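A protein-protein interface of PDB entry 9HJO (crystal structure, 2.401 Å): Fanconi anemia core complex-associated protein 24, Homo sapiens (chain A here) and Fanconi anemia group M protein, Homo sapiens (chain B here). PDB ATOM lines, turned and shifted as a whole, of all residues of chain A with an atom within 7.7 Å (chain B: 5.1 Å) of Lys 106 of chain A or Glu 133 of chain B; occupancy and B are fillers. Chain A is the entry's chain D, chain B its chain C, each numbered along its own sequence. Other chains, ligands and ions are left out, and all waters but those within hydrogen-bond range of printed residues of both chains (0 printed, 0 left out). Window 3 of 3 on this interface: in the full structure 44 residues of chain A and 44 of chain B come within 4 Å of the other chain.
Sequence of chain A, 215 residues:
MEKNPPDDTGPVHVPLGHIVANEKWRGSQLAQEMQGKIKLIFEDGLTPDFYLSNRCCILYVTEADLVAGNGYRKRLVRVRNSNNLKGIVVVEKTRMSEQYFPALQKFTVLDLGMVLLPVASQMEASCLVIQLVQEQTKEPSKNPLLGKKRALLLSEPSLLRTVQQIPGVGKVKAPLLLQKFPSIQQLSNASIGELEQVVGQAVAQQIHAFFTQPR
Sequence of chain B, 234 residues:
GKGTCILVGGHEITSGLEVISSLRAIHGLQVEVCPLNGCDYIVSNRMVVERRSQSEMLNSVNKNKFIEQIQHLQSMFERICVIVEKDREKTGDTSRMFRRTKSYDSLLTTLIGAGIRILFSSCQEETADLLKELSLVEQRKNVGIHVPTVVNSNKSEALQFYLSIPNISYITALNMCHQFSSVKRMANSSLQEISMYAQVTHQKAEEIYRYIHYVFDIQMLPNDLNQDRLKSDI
NZ of Lys 106 of chain A lies within salt-bridge range of OD2 of Asp 129 of chain B (2.7 Å). The side-chain amino group of Lys 106 of chain A lies within salt-bridge range of the side-chain carboxylate of Glu 133 of chain B.
The side-chain carboxylate of Asp 129 of chain B lies within salt-bridge range of the side-chain amino group of Lys 132 of chain B (3.4 Å). The side-chain amino group (NZ) of Lys 132 of chain B is in salt-bridge range of the side-chain carboxylate (OE2) of Glu 133 of chain B (3.2 Å). O of Lys 106 of chain A lies within hydrogen-bond range of N of Asp 111 of chain A.
Gln 105 of chain A touches Leu 130 of chain B (NE2 to CD2, 3.8 Å). CD1 of Leu 110 of chain A touches CB of Glu 133 of chain B, 3.7 Å away. Leu 110 of chain A touches Leu 134 of chain B (CD2 to CD2, 3.7 Å).
Leu 104 of chain A touches none of the printed residues of chain B. Lys 106 of chain A touches just these residues of chain B: Asp 129 (2.7 Å) and Glu 133 (2.8 Å). Printed residues of chain B within 4 Å of Leu 110 of chain A: Glu 133 and Leu 134. Of the printed residues of chain A, Asp 129 of chain B touches Lys 106 (2.7 Å). Of the printed residues of chain A, Leu 130 of chain B touches Gln 105 (3.8 Å). Of chain A, only Lys 106 (2.8 Å) and Leu 110 (3.7 Å) come within 4 Å of Glu 133 of chain B. Of the printed residues of chain A, Leu 134 of chain B touches Leu 110 (3.7 Å). The nearest residue of chain A that does not touch Glu 133 of chain B is Asp 111 of chain A (6.8 Å). The nearest printed residue of chain A that does not touch Asp 129 of chain B is Pro 102 of chain A (5.9 Å).
Of the 9 printed residues of chain B, 4 touch a printed residue of chain A. Hydrophobic or aromatic side chains of chain B within 4 Å of the printed part of chain A: Leu 130 and Leu 134. Printed residues of chain A that touch a printed residue of chain B: Gln 105, Lys 106 and Leu 110. Among the printed residues, 5 pairs touch across the chains. Among the printed residues, Asp or Glu carboxylates within 4 Å of a Lys or Arg side-chain nitrogen of the other chain: Lys 106 of chain A with Asp 129 of chain B (2.7 Å) and Lys 106 of chain A with Glu 133 of chain B (2.8 Å).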
ATOM      1  N   TYR A  72     -13.783  -6.105 -16.308  1.00  0.00           N
ATOM      2  CA  TYR A  72     -14.278  -4.986 -15.510  1.00  0.00           C
ATOM      3  C   TYR A  72     -13.287  -4.565 -14.417  1.00  0.00           C
ATOM      4  O   TYR A  72     -13.243  -3.370 -14.112  1.00  0.00           O
ATOM      5  CB  TYR A  72     -15.652  -5.295 -14.883  1.00  0.00           C
ATOM      6  CG  TYR A  72     -15.652  -6.382 -13.810  1.00  0.00           C
ATOM      7  CD1 TYR A  72     -15.725  -7.732 -14.155  1.00  0.00           C
ATOM      8  CD2 TYR A  72     -15.546  -6.069 -12.462  1.00  0.00           C
ATOM      9  CE1 TYR A  72     -15.702  -8.736 -13.201  1.00  0.00           C
ATOM     10  CE2 TYR A  72     -15.505  -7.063 -11.497  1.00  0.00           C
ATOM     11  CZ  TYR A  72     -15.591  -8.398 -11.865  1.00  0.00           C
ATOM     12  OH  TYR A  72     -15.557  -9.406 -10.946  1.00  0.00           O
ATOM     13  N   ARG A  73     -12.525  -5.528 -13.840  1.00  0.00           N
ATOM     14  CA  ARG A  73     -11.760  -5.328 -12.609  1.00  0.00           C
ATOM     15  C   ARG A  73     -10.618  -4.326 -12.783  1.00  0.00           C
ATOM     16  O   ARG A  73     -10.410  -3.489 -11.905  1.00  0.00           O
ATOM     17  CB  ARG A  73     -11.163  -6.623 -12.041  1.00  0.00           C
ATOM     18  CG  ARG A  73     -12.180  -7.600 -11.477  1.00  0.00           C
ATOM     19  CD  ARG A  73     -11.536  -8.827 -10.852  1.00  0.00           C
ATOM     20  NE  ARG A  73     -12.542  -9.808 -10.426  1.00  0.00           N
ATOM     21  CZ  ARG A  73     -12.329 -10.938  -9.740  1.00  0.00           C
ATOM     22  NH1 ARG A  73     -11.122 -11.279  -9.326  1.00  0.00           N
ATOM     23  NH2 ARG A  73     -13.341 -11.741  -9.462  1.00  0.00           N
ATOM     24  N   TYR A 100     -22.649 -14.719 -11.746  1.00  0.00           N
ATOM     25  CA  TYR A 100     -21.351 -14.062 -11.715  1.00  0.00           C
ATOM     26  C   TYR A 100     -21.250 -12.996 -10.614  1.00  0.00           C
ATOM     27  O   TYR A 100     -20.137 -12.631 -10.246  1.00  0.00           O
ATOM     28  CB  TYR A 100     -21.132 -13.474 -13.114  1.00  0.00           C
ATOM     29  CG  TYR A 100     -21.033 -14.481 -14.254  1.00  0.00           C
ATOM     30  CD1 TYR A 100     -20.270 -15.649 -14.145  1.00  0.00           C
ATOM     31  CD2 TYR A 100     -21.700 -14.259 -15.458  1.00  0.00           C
ATOM     32  CE1 TYR A 100     -20.166 -16.553 -15.193  1.00  0.00           C
ATOM     33  CE2 TYR A 100     -21.616 -15.163 -16.507  1.00  0.00           C
ATOM     34  CZ  TYR A 100     -20.843 -16.307 -16.378  1.00  0.00           C
ATOM     35  OH  TYR A 100     -20.762 -17.179 -17.428  1.00  0.00           O
ATOM     36  N   PHE A 101     -22.388 -12.531 -10.065  1.00  0.00           N
ATOM     37  CA  PHE A 101     -22.443 -11.406  -9.144  1.00  0.00           C
ATOM     38  C   PHE A 101     -21.715 -11.701  -7.833  1.00  0.00           C
ATOM     39  O   PHE A 101     -21.069 -10.792  -7.301  1.00  0.00           O
ATOM     40  CB  PHE A 101     -23.890 -10.974  -8.881  1.00  0.00           C
ATOM     41  CG  PHE A 101     -24.036  -9.865  -7.848  1.00  0.00           C
ATOM     42  CD1 PHE A 101     -24.107 -10.174  -6.488  1.00  0.00           C
ATOM     43  CD2 PHE A 101     -24.088  -8.524  -8.228  1.00  0.00           C
ATOM     44  CE1 PHE A 101     -24.180  -9.167  -5.538  1.00  0.00           C
ATOM     45  CE2 PHE A 101     -24.202  -7.523  -7.265  1.00  0.00           C
ATOM     46  CZ  PHE A 101     -24.237  -7.840  -5.926  1.00  0.00           C
ATOM     47  N   PRO A 102     -21.853 -12.904  -7.220  1.00  0.00           N
ATOM     48  CA  PRO A 102     -21.108 -13.225  -6.008  1.00  0.00           C
ATOM     49  C   PRO A 102     -19.603 -12.970  -6.110  1.00  0.00           C
ATOM     50  O   PRO A 102     -19.051 -12.276  -5.252  1.00  0.00           O
ATOM     51  CB  PRO A 102     -21.419 -14.700  -5.777  1.00  0.00           C
ATOM     52  CG  PRO A 102     -22.753 -14.895  -6.461  1.00  0.00           C
ATOM     53  CD  PRO A 102     -22.763 -13.985  -7.624  1.00  0.00           C
ATOM     54  N   ALA A 103     -18.979 -13.503  -7.182  1.00  0.00           N
ATOM     55  CA  ALA A 103     -17.560 -13.340  -7.485  1.00  0.00           C
ATOM     56  C   ALA A 103     -17.170 -11.869  -7.631  1.00  0.00           C
ATOM     57  O   ALA A 103     -16.130 -11.474  -7.129  1.00  0.00           O
ATOM     58  CB  ALA A 103     -17.203 -14.106  -8.748  1.00  0.00           C
ATOM     59  N   LEU A 104     -17.983 -11.071  -8.330  1.00  0.00           N
ATOM     60  CA  LEU A 104     -17.763  -9.635  -8.436  1.00  0.00           C
ATOM     61  C   LEU A 104     -17.824  -8.966  -7.065  1.00  0.00           C
ATOM     62  O   LEU A 104     -16.984  -8.116  -6.759  1.00  0.00           O
ATOM     63  CB  LEU A 104     -18.756  -8.981  -9.398  1.00  0.00           C
ATOM     64  CG  LEU A 104     -18.544  -7.487  -9.649  1.00  0.00           C
ATOM     65  CD1 LEU A 104     -19.005  -7.200 -11.052  1.00  0.00           C
ATOM     66  CD2 LEU A 104     -19.271  -6.571  -8.696  1.00  0.00           C
ATOM     67  N   GLN A 105     -18.849  -9.302  -6.273  1.00  0.00           N
ATOM     68  CA  GLN A 105     -19.099  -8.613  -5.025  1.00  0.00           C
ATOM     69  C   GLN A 105     -17.997  -8.897  -4.020  1.00  0.00           C
ATOM     70  O   GLN A 105     -17.634  -7.997  -3.263  1.00  0.00           O
ATOM     71  CB  GLN A 105     -20.432  -9.053  -4.431  1.00  0.00           C
ATOM     72  CG  GLN A 105     -20.816  -8.336  -3.144  1.00  0.00           C
ATOM     73  CD  GLN A 105     -22.215  -8.697  -2.714  1.00  0.00           C
ATOM     74  OE1 GLN A 105     -23.097  -7.838  -2.614  1.00  0.00           O
ATOM     75  NE2 GLN A 105     -22.437  -9.983  -2.474  1.00  0.00           N
ATOM     76  N   LYS A 106     -17.539 -10.154  -3.986  1.00  0.00           N
ATOM     77  CA  LYS A 106     -16.393 -10.552  -3.184  1.00  0.00           C
ATOM     78  C   LYS A 106     -15.228  -9.639  -3.525  1.00  0.00           C
ATOM     79  O   LYS A 106     -14.660  -9.029  -2.625  1.00  0.00           O
ATOM     80  CB  LYS A 106     -15.995 -12.017  -3.401  1.00  0.00           C
ATOM     81  CG  LYS A 106     -16.932 -13.018  -2.747  1.00  0.00           C
ATOM     82  CD  LYS A 106     -16.839 -14.431  -3.320  1.00  0.00           C
ATOM     83  CE  LYS A 106     -17.784 -15.407  -2.644  1.00  0.00           C
ATOM     84  NZ  LYS A 106     -17.475 -15.694  -1.235  1.00  0.00           N
ATOM     85  N   PHE A 107     -14.947  -9.506  -4.830  1.00  0.00           N
ATOM     86  CA  PHE A 107     -13.835  -8.702  -5.301  1.00  0.00           C
ATOM     87  C   PHE A 107     -14.037  -7.228  -4.943  1.00  0.00           C
ATOM     88  O   PHE A 107     -13.169  -6.622  -4.328  1.00  0.00           O
ATOM     89  CB  PHE A 107     -13.635  -8.918  -6.803  1.00  0.00           C
ATOM     90  CG  PHE A 107     -12.456  -8.102  -7.315  1.00  0.00           C
ATOM     91  CD1 PHE A 107     -11.149  -8.521  -7.073  1.00  0.00           C
ATOM     92  CD2 PHE A 107     -12.657  -6.884  -7.964  1.00  0.00           C
ATOM     93  CE1 PHE A 107     -10.072  -7.762  -7.500  1.00  0.00           C
ATOM     94  CE2 PHE A 107     -11.576  -6.133  -8.396  1.00  0.00           C
ATOM     95  CZ  PHE A 107     -10.285  -6.568  -8.159  1.00  0.00           C
ATOM     96  N   THR A 108     -15.174  -6.650  -5.347  1.00  0.00           N
ATOM     97  CA  THR A 108     -15.405  -5.218  -5.222  1.00  0.00           C
ATOM     98  C   THR A 108     -15.479  -4.804  -3.756  1.00  0.00           C
ATOM     99  O   THR A 108     -14.857  -3.821  -3.357  1.00  0.00           O
ATOM    100  CB  THR A 108     -16.691  -4.816  -5.943  1.00  0.00           C
ATOM    101  OG1 THR A 108     -16.618  -5.375  -7.255  1.00  0.00           O
ATOM    102  CG2 THR A 108     -16.850  -3.306  -5.998  1.00  0.00           C
ATOM    103  N   VAL A 109     -16.302  -5.519  -2.981  1.00  0.00           N
ATOM    104  CA  VAL A 109     -16.616  -5.074  -1.639  1.00  0.00           C
ATOM    105  C   VAL A 109     -15.526  -5.541  -0.683  1.00  0.00           C
ATOM    106  O   VAL A 109     -15.072  -4.730   0.107  1.00  0.00           O
ATOM    107  CB  VAL A 109     -18.015  -5.454  -1.131  1.00  0.00           C
ATOM    108  CG1 VAL A 109     -18.328  -4.721   0.174  1.00  0.00           C
ATOM    109  CG2 VAL A 109     -19.097  -5.151  -2.164  1.00  0.00           C
ATOM    110  N   LEU A 110     -15.111  -6.814  -0.755  1.00  0.00           N
ATOM    111  CA  LEU A 110     -14.299  -7.411   0.302  1.00  0.00           C
ATOM    112  C   LEU A 110     -12.801  -7.287   0.019  1.00  0.00           C
ATOM    113  O   LEU A 110     -12.075  -6.907   0.921  1.00  0.00           O
ATOM    114  CB  LEU A 110     -14.740  -8.840   0.615  1.00  0.00           C
ATOM    115  CG  LEU A 110     -16.215  -8.968   1.034  1.00  0.00           C
ATOM    116  CD1 LEU A 110     -16.603 -10.414   1.214  1.00  0.00           C
ATOM    117  CD2 LEU A 110     -16.559  -8.201   2.305  1.00  0.00           C
ATOM    118  N   ASP A 111     -12.324  -7.561  -1.201  1.00  0.00           N
ATOM    119  CA  ASP A 111     -10.943  -7.268  -1.554  1.00  0.00           C
ATOM    120  C   ASP A 111     -10.713  -5.758  -1.572  1.00  0.00           C
ATOM    121  O   ASP A 111     -10.051  -5.252  -0.677  1.00  0.00           O
ATOM    122  CB  ASP A 111     -10.506  -7.877  -2.874  1.00  0.00           C
ATOM    123  CG  ASP A 111     -10.535  -9.393  -2.953  1.00  0.00           C
ATOM    124  OD1 ASP A 111     -11.203 -10.009  -2.102  1.00  0.00           O
ATOM    125  OD2 ASP A 111      -9.870  -9.937  -3.861  1.00  0.00           O
ATOM    126  N   LEU A 112     -11.305  -5.042  -2.536  1.00  0.00           N
ATOM    127  CA  LEU A 112     -10.954  -3.655  -2.809  1.00  0.00           C
ATOM    128  C   LEU A 112     -11.551  -2.677  -1.800  1.00  0.00           C
ATOM    129  O   LEU A 112     -11.071  -1.554  -1.719  1.00  0.00           O
ATOM    130  CB  LEU A 112     -11.372  -3.244  -4.220  1.00  0.00           C
ATOM    131  CG  LEU A 112     -10.744  -4.003  -5.393  1.00  0.00           C
ATOM    132  CD1 LEU A 112     -11.264  -3.359  -6.672  1.00  0.00           C
ATOM    133  CD2 LEU A 112      -9.222  -4.016  -5.351  1.00  0.00           C
ATOM    134  N   GLY A 113     -12.604  -3.045  -1.074  1.00  0.00           N
ATOM    135  CA  GLY A 113     -13.172  -2.155  -0.071  1.00  0.00           C
ATOM    136  C   GLY A 113     -14.158  -1.129  -0.629  1.00  0.00           C
ATOM    137  O   GLY A 113     -14.598  -0.269   0.134  1.00  0.00           O
ATOM    138  N   LEU A 116     -20.701  -1.325  -3.667  1.00  0.00           N
ATOM    139  CA  LEU A 116     -21.323  -2.019  -4.786  1.00  0.00           C
ATOM    140  C   LEU A 116     -22.839  -1.923  -4.632  1.00  0.00           C
ATOM    141  O   LEU A 116     -23.347  -2.248  -3.565  1.00  0.00           O
ATOM    142  CB  LEU A 116     -20.893  -3.480  -4.818  1.00  0.00           C
ATOM    143  CG  LEU A 116     -21.455  -4.344  -5.955  1.00  0.00           C
ATOM    144  CD1 LEU A 116     -20.850  -3.949  -7.281  1.00  0.00           C
ATOM    145  CD2 LEU A 116     -21.201  -5.807  -5.640  1.00  0.00           C
ATOM    146  N   ASP B 129     -22.315 -17.765   3.062  1.00  0.00           N
ATOM    147  CA  ASP B 129     -21.025 -17.621   2.418  1.00  0.00           C
ATOM    148  C   ASP B 129     -20.439 -16.240   2.728  1.00  0.00           C
ATOM    149  O   ASP B 129     -19.273 -16.121   3.081  1.00  0.00           O
ATOM    150  CB  ASP B 129     -21.132 -18.004   0.954  1.00  0.00           C
ATOM    151  CG  ASP B 129     -19.818 -17.970   0.191  1.00  0.00           C
ATOM    152  OD1 ASP B 129     -18.940 -18.817   0.476  1.00  0.00           O
ATOM    153  OD2 ASP B 129     -19.677 -17.075  -0.671  1.00  0.00           O
ATOM    154  N   LEU B 130     -21.247 -15.192   2.633  1.00  0.00           N
ATOM    155  CA  LEU B 130     -20.789 -13.850   2.947  1.00  0.00           C
ATOM    156  C   LEU B 130     -20.409 -13.743   4.425  1.00  0.00           C
ATOM    157  O   LEU B 130     -19.395 -13.126   4.757  1.00  0.00           O
ATOM    158  CB  LEU B 130     -21.867 -12.832   2.576  1.00  0.00           C
ATOM    159  CG  LEU B 130     -22.146 -12.651   1.080  1.00  0.00           C
ATOM    160  CD1 LEU B 130     -23.391 -11.784   0.940  1.00  0.00           C
ATOM    161  CD2 LEU B 130     -20.991 -12.053   0.304  1.00  0.00           C
ATOM    162  N   LEU B 131     -21.225 -14.332   5.308  1.00  0.00           N
ATOM    163  CA  LEU B 131     -20.939 -14.319   6.732  1.00  0.00           C
ATOM    164  C   LEU B 131     -19.576 -14.949   7.013  1.00  0.00           C
ATOM    165  O   LEU B 131     -18.855 -14.438   7.854  1.00  0.00           O
ATOM    166  CB  LEU B 131     -22.061 -14.989   7.520  1.00  0.00           C
ATOM    167  CG  LEU B 131     -23.305 -14.128   7.742  1.00  0.00           C
ATOM    168  CD1 LEU B 131     -24.440 -14.960   8.313  1.00  0.00           C
ATOM    169  CD2 LEU B 131     -23.024 -12.927   8.637  1.00  0.00           C
ATOM    170  N   LYS B 132     -19.218 -16.012   6.273  1.00  0.00           N
ATOM    171  CA  LYS B 132     -17.973 -16.736   6.449  1.00  0.00           C
ATOM    172  C   LYS B 132     -16.812 -15.879   5.982  1.00  0.00           C
ATOM    173  O   LYS B 132     -15.798 -15.859   6.671  1.00  0.00           O
ATOM    174  CB  LYS B 132     -17.944 -18.085   5.711  1.00  0.00           C
ATOM    175  CG  LYS B 132     -16.599 -18.825   5.640  1.00  0.00           C
ATOM    176  CD  LYS B 132     -15.845 -18.649   4.326  1.00  0.00           C
ATOM    177  CE  LYS B 132     -16.431 -19.420   3.175  1.00  0.00           C
ATOM    178  NZ  LYS B 132     -15.845 -19.029   1.890  1.00  0.00           N
ATOM    179  N   GLU B 133     -16.948 -15.249   4.805  1.00  0.00           N
ATOM    180  CA  GLU B 133     -15.936 -14.353   4.271  1.00  0.00           C
ATOM    181  C   GLU B 133     -15.681 -13.203   5.234  1.00  0.00           C
ATOM    182  O   GLU B 133     -14.534 -12.852   5.492  1.00  0.00           O
ATOM    183  CB  GLU B 133     -16.355 -13.690   2.967  1.00  0.00           C
ATOM    184  CG  GLU B 133     -16.430 -14.658   1.790  1.00  0.00           C
ATOM    185  CD  GLU B 133     -15.149 -15.307   1.298  1.00  0.00           C
ATOM    186  OE1 GLU B 133     -14.048 -14.894   1.710  1.00  0.00           O
ATOM    187  OE2 GLU B 133     -15.289 -16.226   0.447  1.00  0.00           O
ATOM    188  N   LEU B 134     -16.762 -12.618   5.748  1.00  0.00           N
ATOM    189  CA  LEU B 134     -16.655 -11.557   6.736  1.00  0.00           C
ATOM    190  C   LEU B 134     -15.945 -12.087   7.979  1.00  0.00           C
ATOM    191  O   LEU B 134     -15.157 -11.369   8.559  1.00  0.00           O
ATOM    192  CB  LEU B 134     -18.034 -10.979   7.066  1.00  0.00           C
ATOM    193  CG  LEU B 134     -18.729 -10.192   5.952  1.00  0.00           C
ATOM    194  CD1 LEU B 134     -20.156  -9.953   6.381  1.00  0.00           C
ATOM    195  CD2 LEU B 134     -18.030  -8.866   5.607  1.00  0.00           C
ATOM    196  N   SER B 135     -16.213 -13.342   8.370  1.00  0.00           N
ATOM    197  CA  SER B 135     -15.557 -13.977   9.506  1.00  0.00           C
ATOM    198  C   SER B 135     -14.035 -14.029   9.312  1.00  0.00           C
ATOM    199  O   SER B 135     -13.319 -13.731  10.254  1.00  0.00           O
ATOM    200  CB  SER B 135     -16.112 -15.343   9.779  1.00  0.00           C
ATOM    201  OG  SER B 135     -15.937 -15.669  11.146  1.00  0.00           O
ATOM    202  N   LEU B 136     -13.586 -14.397   8.100  1.00  0.00           N
ATOM    203  CA  LEU B 136     -12.183 -14.541   7.745  1.00  0.00           C
ATOM    204  C   LEU B 136     -11.438 -13.208   7.877  1.00  0.00           C
ATOM    205  O   LEU B 136     -10.360 -13.171   8.456  1.00  0.00           O
ATOM    206  CB  LEU B 136     -12.014 -15.103   6.330  1.00  0.00           C
ATOM    207  CG  LEU B 136     -12.351 -16.584   6.111  1.00  0.00           C
ATOM    208  CD1 LEU B 136     -12.062 -16.976   4.654  1.00  0.00           C
ATOM    209  CD2 LEU B 136     -11.617 -17.519   7.052  1.00  0.00           C
ATOM    210  N   VAL B 137     -11.992 -12.131   7.316  1.00  0.00           N
ATOM    211  CA  VAL B 137     -11.379 -10.808   7.327  1.00  0.00           C
ATOM    212  C   VAL B 137     -11.107 -10.398   8.771  1.00  0.00           C
ATOM    213  O   VAL B 137     -10.018  -9.936   9.101  1.00  0.00           O
ATOM    214  CB  VAL B 137     -12.248  -9.745   6.631  1.00  0.00           C
ATOM    215  CG1 VAL B 137     -11.663  -8.335   6.781  1.00  0.00           C
ATOM    216  CG2 VAL B 137     -12.465 -10.071   5.159  1.00  0.00           C
